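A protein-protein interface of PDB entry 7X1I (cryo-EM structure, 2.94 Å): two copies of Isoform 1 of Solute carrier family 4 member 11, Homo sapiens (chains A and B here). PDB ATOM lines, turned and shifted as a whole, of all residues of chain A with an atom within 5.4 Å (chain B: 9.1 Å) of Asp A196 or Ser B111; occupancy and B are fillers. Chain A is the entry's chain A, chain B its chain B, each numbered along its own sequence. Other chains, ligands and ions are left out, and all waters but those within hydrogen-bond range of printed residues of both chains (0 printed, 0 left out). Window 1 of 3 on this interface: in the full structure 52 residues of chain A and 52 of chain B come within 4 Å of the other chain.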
ATOM      1  N   HIS A 109     -15.169 -23.881 -17.523  1.00  0.00           N
ATOM      2  CA  HIS A 109     -14.404 -24.680 -18.469  1.00  0.00           C
ATOM      3  C   HIS A 109     -14.475 -24.026 -19.842  1.00  0.00           C
ATOM      4  O   HIS A 109     -15.564 -23.869 -20.404  1.00  0.00           O
ATOM      5  CB  HIS A 109     -14.933 -26.113 -18.529  1.00  0.00           C
ATOM      6  CG  HIS A 109     -14.221 -26.979 -19.521  1.00  0.00           C
ATOM      7  ND1 HIS A 109     -14.823 -28.057 -20.134  1.00  0.00           N
ATOM      8  CD2 HIS A 109     -12.958 -26.927 -20.007  1.00  0.00           C
ATOM      9  CE1 HIS A 109     -13.962 -28.632 -20.955  1.00  0.00           C
ATOM     10  NE2 HIS A 109     -12.823 -27.965 -20.897  1.00  0.00           N
ATOM     11  N   THR A 110     -13.318 -23.646 -20.379  1.00  0.00           N
ATOM     12  CA  THR A 110     -13.222 -23.038 -21.699  1.00  0.00           C
ATOM     13  C   THR A 110     -12.503 -24.007 -22.628  1.00  0.00           C
ATOM     14  O   THR A 110     -11.369 -24.413 -22.352  1.00  0.00           O
ATOM     15  CB  THR A 110     -12.483 -21.700 -21.640  1.00  0.00           C
ATOM     16  OG1 THR A 110     -13.165 -20.815 -20.740  1.00  0.00           O
ATOM     17  CG2 THR A 110     -12.425 -21.064 -23.021  1.00  0.00           C
ATOM     18  N   SER A 111     -13.164 -24.373 -23.724  1.00  0.00           N
ATOM     19  CA  SER A 111     -12.606 -25.284 -24.715  1.00  0.00           C
ATOM     20  C   SER A 111     -12.518 -24.561 -26.051  1.00  0.00           C
ATOM     21  O   SER A 111     -13.532 -24.080 -26.568  1.00  0.00           O
ATOM     22  CB  SER A 111     -13.459 -26.550 -24.840  1.00  0.00           C
ATOM     23  OG  SER A 111     -12.913 -27.438 -25.800  1.00  0.00           O
ATOM     24  N   ARG A 112     -11.310 -24.484 -26.601  1.00  0.00           N
ATOM     25  CA  ARG A 112     -11.065 -23.829 -27.878  1.00  0.00           C
ATOM     26  C   ARG A 112     -10.632 -24.871 -28.901  1.00  0.00           C
ATOM     27  O   ARG A 112      -9.670 -25.611 -28.671  1.00  0.00           O
ATOM     28  CB  ARG A 112      -9.998 -22.742 -27.738  1.00  0.00           C
ATOM     29  CG  ARG A 112     -10.304 -21.726 -26.652  1.00  0.00           C
ATOM     30  CD  ARG A 112      -9.149 -20.761 -26.454  1.00  0.00           C
ATOM     31  NE  ARG A 112      -9.419 -19.802 -25.388  1.00  0.00           N
ATOM     32  CZ  ARG A 112      -9.141 -20.008 -24.108  1.00  0.00           C
ATOM     33  NH1 ARG A 112      -8.588 -21.136 -23.694  1.00  0.00           N
ATOM     34  NH2 ARG A 112      -9.426 -19.059 -23.222  1.00  0.00           N
ATOM     35  N   LEU A 179     -28.166 -17.802 -23.982  1.00  0.00           N
ATOM     36  CA  LEU A 179     -26.978 -17.391 -24.725  1.00  0.00           C
ATOM     37  C   LEU A 179     -25.731 -17.406 -23.846  1.00  0.00           C
ATOM     38  O   LEU A 179     -24.665 -17.859 -24.278  1.00  0.00           O
ATOM     39  CB  LEU A 179     -27.193 -15.999 -25.321  1.00  0.00           C
ATOM     40  CG  LEU A 179     -28.135 -15.914 -26.524  1.00  0.00           C
ATOM     41  CD1 LEU A 179     -28.666 -14.500 -26.696  1.00  0.00           C
ATOM     42  CD2 LEU A 179     -27.410 -16.362 -27.776  1.00  0.00           C
ATOM     43  N   LEU A 194     -20.173 -15.613 -23.015  1.00  0.00           N
ATOM     44  CA  LEU A 194     -20.955 -16.319 -24.020  1.00  0.00           C
ATOM     45  C   LEU A 194     -20.598 -17.801 -24.033  1.00  0.00           C
ATOM     46  O   LEU A 194     -19.421 -18.169 -23.971  1.00  0.00           O
ATOM     47  CB  LEU A 194     -20.721 -15.697 -25.398  1.00  0.00           C
ATOM     48  CG  LEU A 194     -21.294 -14.293 -25.604  1.00  0.00           C
ATOM     49  CD1 LEU A 194     -20.775 -13.666 -26.890  1.00  0.00           C
ATOM     50  CD2 LEU A 194     -22.815 -14.336 -25.610  1.00  0.00           C
ATOM     51  N   SER A 195     -21.625 -18.653 -24.108  1.00  0.00           N
ATOM     52  CA  SER A 195     -21.399 -20.095 -24.048  1.00  0.00           C
ATOM     53  C   SER A 195     -20.629 -20.597 -25.266  1.00  0.00           C
ATOM     54  O   SER A 195     -19.666 -21.358 -25.125  1.00  0.00           O
ATOM     55  CB  SER A 195     -22.732 -20.831 -23.921  1.00  0.00           C
ATOM     56  OG  SER A 195     -22.536 -22.234 -23.881  1.00  0.00           O
ATOM     57  N   ASP A 196     -21.036 -20.182 -26.464  1.00  0.00           N
ATOM     58  CA  ASP A 196     -20.421 -20.656 -27.696  1.00  0.00           C
ATOM     59  C   ASP A 196     -20.210 -19.490 -28.646  1.00  0.00           C
ATOM     60  O   ASP A 196     -21.126 -18.696 -28.881  1.00  0.00           O
ATOM     61  CB  ASP A 196     -21.282 -21.727 -28.376  1.00  0.00           C
ATOM     62  CG  ASP A 196     -21.386 -22.999 -27.558  1.00  0.00           C
ATOM     63  OD1 ASP A 196     -20.370 -23.399 -26.954  1.00  0.00           O
ATOM     64  OD2 ASP A 196     -22.482 -23.598 -27.519  1.00  0.00           O
ATOM     65  N   THR A 197     -19.008 -19.410 -29.212  1.00  0.00           N
ATOM     66  CA  THR A 197     -18.669 -18.364 -30.163  1.00  0.00           C
ATOM     67  C   THR A 197     -17.707 -18.923 -31.198  1.00  0.00           C
ATOM     68  O   THR A 197     -16.998 -19.904 -30.955  1.00  0.00           O
ATOM     69  CB  THR A 197     -18.042 -17.142 -29.475  1.00  0.00           C
ATOM     70  OG1 THR A 197     -17.082 -17.578 -28.505  1.00  0.00           O
ATOM     71  CG2 THR A 197     -19.103 -16.295 -28.795  1.00  0.00           C
ATOM     72  N   ILE A 198     -17.698 -18.287 -32.366  1.00  0.00           N
ATOM     73  CA  ILE A 198     -16.755 -18.589 -33.435  1.00  0.00           C
ATOM     74  C   ILE A 198     -16.094 -17.286 -33.858  1.00  0.00           C
ATOM     75  O   ILE A 198     -16.784 -16.306 -34.159  1.00  0.00           O
ATOM     76  CB  ILE A 198     -17.443 -19.270 -34.632  1.00  0.00           C
ATOM     77  CG1 ILE A 198     -17.840 -20.703 -34.279  1.00  0.00           C
ATOM     78  CG2 ILE A 198     -16.535 -19.258 -35.851  1.00  0.00           C
ATOM     79  CD1 ILE A 198     -18.369 -21.492 -35.458  1.00  0.00           C
ATOM     80  N   CYS A 216     -19.324 -14.205 -34.081  1.00  0.00           N
ATOM     81  CA  CYS A 216     -20.440 -15.104 -34.334  1.00  0.00           C
ATOM     82  C   CYS A 216     -20.878 -15.731 -33.018  1.00  0.00           C
ATOM     83  O   CYS A 216     -20.051 -16.275 -32.280  1.00  0.00           O
ATOM     84  CB  CYS A 216     -20.056 -16.192 -35.342  1.00  0.00           C
ATOM     85  SG  CYS A 216     -21.399 -17.318 -35.775  1.00  0.00           S
ATOM     86  N   ILE A 217     -22.175 -15.654 -32.730  1.00  0.00           N
ATOM     87  CA  ILE A 217     -22.747 -16.161 -31.490  1.00  0.00           C
ATOM     88  C   ILE A 217     -23.677 -17.321 -31.818  1.00  0.00           C
ATOM     89  O   ILE A 217     -24.489 -17.236 -32.747  1.00  0.00           O
ATOM     90  CB  ILE A 217     -23.489 -15.051 -30.720  1.00  0.00           C
ATOM     91  CG1 ILE A 217     -22.533 -13.895 -30.420  1.00  0.00           C
ATOM     92  CG2 ILE A 217     -24.088 -15.595 -29.433  1.00  0.00           C
ATOM     93  CD1 ILE A 217     -23.164 -12.768 -29.646  1.00  0.00           C
ATOM     94  N   ILE A 218     -23.551 -18.408 -31.056  1.00  0.00           N
ATOM     95  CA  ILE A 218     -24.261 -19.655 -31.314  1.00  0.00           C
ATOM     96  C   ILE A 218     -24.998 -20.076 -30.049  1.00  0.00           C
ATOM     97  O   ILE A 218     -24.443 -20.019 -28.947  1.00  0.00           O
ATOM     98  CB  ILE A 218     -23.292 -20.770 -31.763  1.00  0.00           C
ATOM     99  CG1 ILE A 218     -22.366 -20.262 -32.868  1.00  0.00           C
ATOM    100  CG2 ILE A 218     -24.057 -21.992 -32.244  1.00  0.00           C
ATOM    101  CD1 ILE A 218     -21.201 -21.171 -33.126  1.00  0.00           C
ATOM    102  N   MET A 266     -23.825 -25.226 -35.005  1.00  0.00           N
ATOM    103  CA  MET A 266     -22.420 -24.989 -35.324  1.00  0.00           C
ATOM    104  C   MET A 266     -22.186 -24.974 -36.831  1.00  0.00           C
ATOM    105  O   MET A 266     -21.431 -24.136 -37.341  1.00  0.00           O
ATOM    106  CB  MET A 266     -21.546 -26.053 -34.658  1.00  0.00           C
ATOM    107  CG  MET A 266     -21.661 -26.123 -33.139  1.00  0.00           C
ATOM    108  SD  MET A 266     -21.048 -24.649 -32.299  1.00  0.00           S
ATOM    109  CE  MET A 266     -19.369 -24.573 -32.919  1.00  0.00           C
ATOM    110  N   LEU B 108     -12.092 -20.316 -35.021  1.00  0.00           N
ATOM    111  CA  LEU B 108     -11.831 -20.755 -33.656  1.00  0.00           C
ATOM    112  C   LEU B 108     -13.154 -20.848 -32.910  1.00  0.00           C
ATOM    113  O   LEU B 108     -13.879 -19.855 -32.797  1.00  0.00           O
ATOM    114  CB  LEU B 108     -10.875 -19.796 -32.947  1.00  0.00           C
ATOM    115  CG  LEU B 108     -10.474 -20.175 -31.521  1.00  0.00           C
ATOM    116  CD1 LEU B 108      -9.732 -21.503 -31.514  1.00  0.00           C
ATOM    117  CD2 LEU B 108      -9.628 -19.082 -30.890  1.00  0.00           C
ATOM    118  N   HIS B 109     -13.463 -22.039 -32.403  1.00  0.00           N
ATOM    119  CA  HIS B 109     -14.677 -22.280 -31.638  1.00  0.00           C
ATOM    120  C   HIS B 109     -14.332 -22.300 -30.154  1.00  0.00           C
ATOM    121  O   HIS B 109     -13.534 -23.132 -29.710  1.00  0.00           O
ATOM    122  CB  HIS B 109     -15.333 -23.596 -32.054  1.00  0.00           C
ATOM    123  CG  HIS B 109     -16.564 -23.932 -31.270  1.00  0.00           C
ATOM    124  ND1 HIS B 109     -16.986 -25.229 -31.068  1.00  0.00           N
ATOM    125  CD2 HIS B 109     -17.463 -23.141 -30.638  1.00  0.00           C
ATOM    126  CE1 HIS B 109     -18.092 -25.223 -30.346  1.00  0.00           C
ATOM    127  NE2 HIS B 109     -18.402 -23.968 -30.071  1.00  0.00           N
ATOM    128  N   THR B 110     -14.931 -21.387 -29.394  1.00  0.00           N
ATOM    129  CA  THR B 110     -14.728 -21.303 -27.953  1.00  0.00           C
ATOM    130  C   THR B 110     -16.029 -21.683 -27.258  1.00  0.00           C
ATOM    131  O   THR B 110     -17.070 -21.062 -27.497  1.00  0.00           O
ATOM    132  CB  THR B 110     -14.284 -19.900 -27.538  1.00  0.00           C
ATOM    133  OG1 THR B 110     -13.073 -19.557 -28.225  1.00  0.00           O
ATOM    134  CG2 THR B 110     -14.044 -19.842 -26.036  1.00  0.00           C
ATOM    135  N   SER B 111     -15.964 -22.700 -26.401  1.00  0.00           N
ATOM    136  CA  SER B 111     -17.119 -23.175 -25.650  1.00  0.00           C
ATOM    137  C   SER B 111     -16.832 -23.027 -24.164  1.00  0.00           C
ATOM    138  O   SER B 111     -15.851 -23.584 -23.660  1.00  0.00           O
ATOM    139  CB  SER B 111     -17.442 -24.631 -25.998  1.00  0.00           C
ATOM    140  OG  SER B 111     -18.569 -25.090 -25.272  1.00  0.00           O
ATOM    141  N   ARG B 112     -17.684 -22.277 -23.470  1.00  0.00           N
ATOM    142  CA  ARG B 112     -17.546 -22.045 -22.039  1.00  0.00           C
ATOM    143  C   ARG B 112     -18.711 -22.701 -21.311  1.00  0.00           C
ATOM    144  O   ARG B 112     -19.876 -22.430 -21.623  1.00  0.00           O
ATOM    145  CB  ARG B 112     -17.499 -20.548 -21.733  1.00  0.00           C
ATOM    146  CG  ARG B 112     -16.432 -19.801 -22.512  1.00  0.00           C
ATOM    147  CD  ARG B 112     -16.524 -18.303 -22.283  1.00  0.00           C
ATOM    148  NE  ARG B 112     -15.526 -17.572 -23.056  1.00  0.00           N
ATOM    149  CZ  ARG B 112     -15.708 -17.143 -24.297  1.00  0.00           C
ATOM    150  NH1 ARG B 112     -16.841 -17.359 -24.944  1.00  0.00           N
ATOM    151  NH2 ARG B 112     -14.727 -16.480 -24.904  1.00  0.00           N
ATOM    152  N   LYS B 113     -18.393 -23.558 -20.344  1.00  0.00           N
ATOM    153  CA  LYS B 113     -19.399 -24.284 -19.585  1.00  0.00           C
ATOM    154  C   LYS B 113     -19.047 -24.244 -18.107  1.00  0.00           C
ATOM    155  O   LYS B 113     -17.887 -24.437 -17.731  1.00  0.00           O
ATOM    156  CB  LYS B 113     -19.513 -25.742 -20.049  1.00  0.00           C
ATOM    157  CG  LYS B 113     -19.894 -25.915 -21.511  1.00  0.00           C
ATOM    158  CD  LYS B 113     -19.974 -27.385 -21.884  1.00  0.00           C
ATOM    159  CE  LYS B 113     -20.296 -27.565 -23.358  1.00  0.00           C
ATOM    160  NZ  LYS B 113     -21.602 -26.948 -23.718  1.00  0.00           N
ATOM    161  N   TYR B 114     -20.053 -23.997 -17.275  1.00  0.00           N
ATOM    162  CA  TYR B 114     -19.851 -24.024 -15.834  1.00  0.00           C
ATOM    163  C   TYR B 114     -19.679 -25.456 -15.346  1.00  0.00           C
ATOM    164  O   TYR B 114     -20.324 -26.383 -15.847  1.00  0.00           O
ATOM    165  CB  TYR B 114     -21.027 -23.366 -15.115  1.00  0.00           C
ATOM    166  CG  TYR B 114     -20.950 -21.856 -15.056  1.00  0.00           C
ATOM    167  CD1 TYR B 114     -19.735 -21.197 -15.186  1.00  0.00           C
ATOM    168  CD2 TYR B 114     -22.093 -21.092 -14.865  1.00  0.00           C
ATOM    169  CE1 TYR B 114     -19.661 -19.816 -15.127  1.00  0.00           C
ATOM    170  CE2 TYR B 114     -22.029 -19.713 -14.806  1.00  0.00           C
ATOM    171  CZ  TYR B 114     -20.811 -19.080 -14.938  1.00  0.00           C
ATOM    172  OH  TYR B 114     -20.744 -17.707 -14.881  1.00  0.00           O
ATOM    173  N   LEU B 194      -4.799 -21.824 -25.442  1.00  0.00           N
ATOM    174  CA  LEU B 194      -4.881 -23.120 -24.783  1.00  0.00           C
ATOM    175  C   LEU B 194      -6.182 -23.825 -25.150  1.00  0.00           C
ATOM    176  O   LEU B 194      -7.253 -23.210 -25.169  1.00  0.00           O
ATOM    177  CB  LEU B 194      -4.771 -22.946 -23.267  1.00  0.00           C
ATOM    178  CG  LEU B 194      -3.403 -22.506 -22.741  1.00  0.00           C
ATOM    179  CD1 LEU B 194      -3.476 -22.100 -21.278  1.00  0.00           C
ATOM    180  CD2 LEU B 194      -2.379 -23.615 -22.936  1.00  0.00           C
ATOM    181  N   SER B 195      -6.083 -25.124 -25.447  1.00  0.00           N
ATOM    182  CA  SER B 195      -7.255 -25.877 -25.888  1.00  0.00           C
ATOM    183  C   SER B 195      -8.294 -26.001 -24.779  1.00  0.00           C
ATOM    184  O   SER B 195      -9.486 -25.768 -25.011  1.00  0.00           O
ATOM    185  CB  SER B 195      -6.836 -27.261 -26.382  1.00  0.00           C
ATOM    186  OG  SER B 195      -7.963 -28.015 -26.796  1.00  0.00           O
ATOM    187  N   ASP B 196      -7.865 -26.363 -23.571  1.00  0.00           N
ATOM    188  CA  ASP B 196      -8.780 -26.584 -22.459  1.00  0.00           C
ATOM    189  C   ASP B 196      -8.216 -25.955 -21.198  1.00  0.00           C
ATOM    190  O   ASP B 196      -7.046 -26.160 -20.861  1.00  0.00           O
ATOM    191  CB  ASP B 196      -9.026 -28.080 -22.224  1.00  0.00           C
ATOM    192  CG  ASP B 196      -9.755 -28.740 -23.377  1.00  0.00           C
ATOM    193  OD1 ASP B 196     -10.669 -28.105 -23.941  1.00  0.00           O
ATOM    194  OD2 ASP B 196      -9.414 -29.892 -23.720  1.00  0.00           O
ATOM    195  N   THR B 197      -9.063 -25.212 -20.489  1.00  0.00           N
ATOM    196  CA  THR B 197      -8.672 -24.568 -19.245  1.00  0.00           C
ATOM    197  C   THR B 197      -9.864 -24.540 -18.303  1.00  0.00           C
ATOM    198  O   THR B 197     -11.022 -24.601 -18.727  1.00  0.00           O
ATOM    199  CB  THR B 197      -8.157 -23.140 -19.474  1.00  0.00           C
ATOM    200  OG1 THR B 197      -9.013 -22.463 -20.402  1.00  0.00           O
ATOM    201  CG2 THR B 197      -6.736 -23.153 -20.010  1.00  0.00           C
ATOM    202  N   TYR B 210     -13.892 -13.247 -12.799  1.00  0.00           N
ATOM    203  CA  TYR B 210     -12.915 -14.320 -12.893  1.00  0.00           C
ATOM    204  C   TYR B 210     -11.894 -14.220 -11.765  1.00  0.00           C
ATOM    205  O   TYR B 210     -11.738 -13.182 -11.116  1.00  0.00           O
ATOM    206  CB  TYR B 210     -12.200 -14.278 -14.244  1.00  0.00           C
ATOM    207  CG  TYR B 210     -13.019 -14.809 -15.397  1.00  0.00           C
ATOM    208  CD1 TYR B 210     -14.028 -14.044 -15.968  1.00  0.00           C
ATOM    209  CD2 TYR B 210     -12.776 -16.071 -15.921  1.00  0.00           C
ATOM    210  CE1 TYR B 210     -14.777 -14.525 -17.025  1.00  0.00           C
ATOM    211  CE2 TYR B 210     -13.519 -16.560 -16.980  1.00  0.00           C
ATOM    212  CZ  TYR B 210     -14.518 -15.783 -17.526  1.00  0.00           C
ATOM    213  OH  TYR B 210     -15.259 -16.267 -18.580  1.00  0.00           O
ATOM    214  N   MET B 266     -10.557 -34.029 -17.233  1.00  0.00           N
ATOM    215  CA  MET B 266     -11.403 -32.970 -16.689  1.00  0.00           C
ATOM    216  C   MET B 266     -11.740 -33.225 -15.223  1.00  0.00           C
ATOM    217  O   MET B 266     -11.732 -32.294 -14.408  1.00  0.00           O
ATOM    218  CB  MET B 266     -12.683 -32.846 -17.518  1.00  0.00           C
ATOM    219  CG  MET B 266     -12.466 -32.540 -18.995  1.00  0.00           C
ATOM    220  SD  MET B 266     -11.743 -30.916 -19.299  1.00  0.00           S
ATOM    221  CE  MET B 266     -12.930 -29.852 -18.482  1.00  0.00           C
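The backbone NH (N) of His A109 is in hydrogen-bond range of the backbone carbonyl oxygen (O) of Lys B113. SD of Met B266 lies close to NE2 of His A109. The backbone NH of Thr A110 sits at hydrogen-bond distance from the backbone carbonyl oxygen of Thr B197 (3.0 Å). The backbone NH (N) of Ser A111 lies within hydrogen-bond range of the backbone carbonyl oxygen (O) of Ser B111, at 2.8 Å. The side-chain carboxylate (OD1) of Asp B196 lies within hydrogen-bond range of the side-chain hydroxyl (OG) of Ser A111, 3.0 Å away. The guanidinium group of Arg A112 sits at hydrogen-bond distance from the backbone carbonyl oxygen of Leu B194, at 2.9 Å. The backbone NH (N) of Arg A112 sits at hydrogen-bond distance from the backbone carbonyl oxygen (O) of Ser B195. The backbone carbonyl oxygen (O) of Leu A194 sits at hydrogen-bond distance from the guanidinium group (NH1) of Arg B112 (2.9 Å). The backbone NH (N) of Arg B112 sits at hydrogen-bond distance from the backbone carbonyl oxygen (O) of Ser A195, 2.7 Å away. OD1 of Asp A196 is in hydrogen-bond range of OG of Ser B111, at 3.0 Å. The backbone carbonyl oxygen of Thr A197 sits at hydrogen-bond distance from the backbone NH of Thr B110 (3.0 Å). A ring nitrogen (NE2) of His B109 sits close to the side-chain sulfur (SD) of Met A266 (3.5 Å). The backbone carbonyl oxygen (O) of His A109 sits close to the backbone carbonyl oxygen (O) of Ser B111, at 3.3 Å. The backbone carbonyl oxygen of His B109 lies close to the backbone carbonyl oxygen of Ser A111 (3.3 Å).
Printed residues of chain B that touch a printed residue of chain A: Leu B108, His B109, Thr B110, Ser B111, Arg B112, Lys B113, Leu B194, Ser B195, Asp B196, Thr B197 and Met B266. Along chain B the printed residues that touch a printed residue of chain A span positions 108 to 266. Hydrophobic or aromatic side chains of chain A within 4 Å of the printed part of chain B: His A109 and Met A266. Among the printed residues, 36 pairs touch across the chains. Among the printed residues, no Asp or Glu carboxylate lies within 4 Å of a Lys or Arg side-chain nitrogen of the other chain.
Of chain B, only Thr B110 (3.6 Å), Ser B111 (3.3 Å), Arg B112 (3.9 Å), Ser B195 (3.5 Å), Asp B196 (3.4 Å) and Thr B197 (3.0 Å) come within 4 Å of Thr A110. Of the printed residues of chain B, Arg A112 touches Leu B108 (3.98 Å), His B109 (3.2 Å), Thr B110 (3.9 Å), Leu B194 (2.9 Å), Ser B195 (2.7 Å) and Thr B197 (3.6 Å). Ser A195 touches just these residues of chain B: Thr B110 (3.5 Å), Ser B111 (3.2 Å) and Arg B112 (2.7 Å). Of the printed residues of chain B, Asp A196 touches His B109, Thr B110 and Ser B111. Of chain B, only Leu B108, His B109, Thr B110 and Arg B112 come within 4 Å of Thr A197. Printed residues of chain B within 4 Å of Ile A198: Leu B108. No residue of chain B comes within 4 Å of Ile A218. Printed residues of chain A within 4 Å of Thr B110: Thr A110, Ser A111, Arg A112, Ser A195, Asp A196 and Thr A197. Of chain A, only His A109 (3.3 Å), Thr A110 (3.3 Å), Ser A111 (2.8 Å), Ser A195 (3.2 Å) and Asp A196 (3.0 Å) come within 4 Å of Ser B111. Of the printed residues of chain A, Leu B194 touches Arg A112. Of the printed residues of chain A, Thr B197 touches His A109, Thr A110 and Arg A112. Tyr B210 touches none of the printed residues of chain A. The nearest residue of chain A that does not touch Ser B111 is Arg A112 (5.0 Å). The nearest printed residue of chain B that does not touch Ile A198 is His B109 (4.4 Å).
His A109 touches Arg B112, and with the chains exchanged Arg A112 touches His B109. Ser A111 touches Asp B196, and with the chains exchanged Asp A196 touches Ser B111. Arg A112 touches Leu B194, and with the chains exchanged Leu A194 touches Arg B112. Arg A112 touches Ser B195, and with the chains exchanged Ser A195 touches Arg B112.
The backbone NH (N) of Ser A195 is in hydrogen-bond range of the backbone carbonyl oxygen (O) of Leu A179, 3.1 Å away. The backbone carbonyl oxygen (O) of Asp A196 is in hydrogen-bond range of the backbone NH (N) of Ile A218 (3.3 Å). N of Ile A198 sits at hydrogen-bond distance from O of Cys A216 (3.1 Å).
Thr B197 touches His A109 (O to CD2, 3.3 Å). Ser B111 touches Thr A110 (O to CA, 3.3 Å). Arg B112 touches Thr A110 (CG to OG1, 3.9 Å). Thr A110 touches Asp B196. Ser B195 touches Ser A111 (O to CA, 3.2 Å). Arg A112 touches His B109 (CA to O, 3.2 Å). Ser A195 touches Thr B110 (O to O, 3.5 Å). Asp A196 touches His B109. Thr A197 touches His B109. Thr A197 touches Arg B112 (OG1 to NH1, 3.6 Å).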
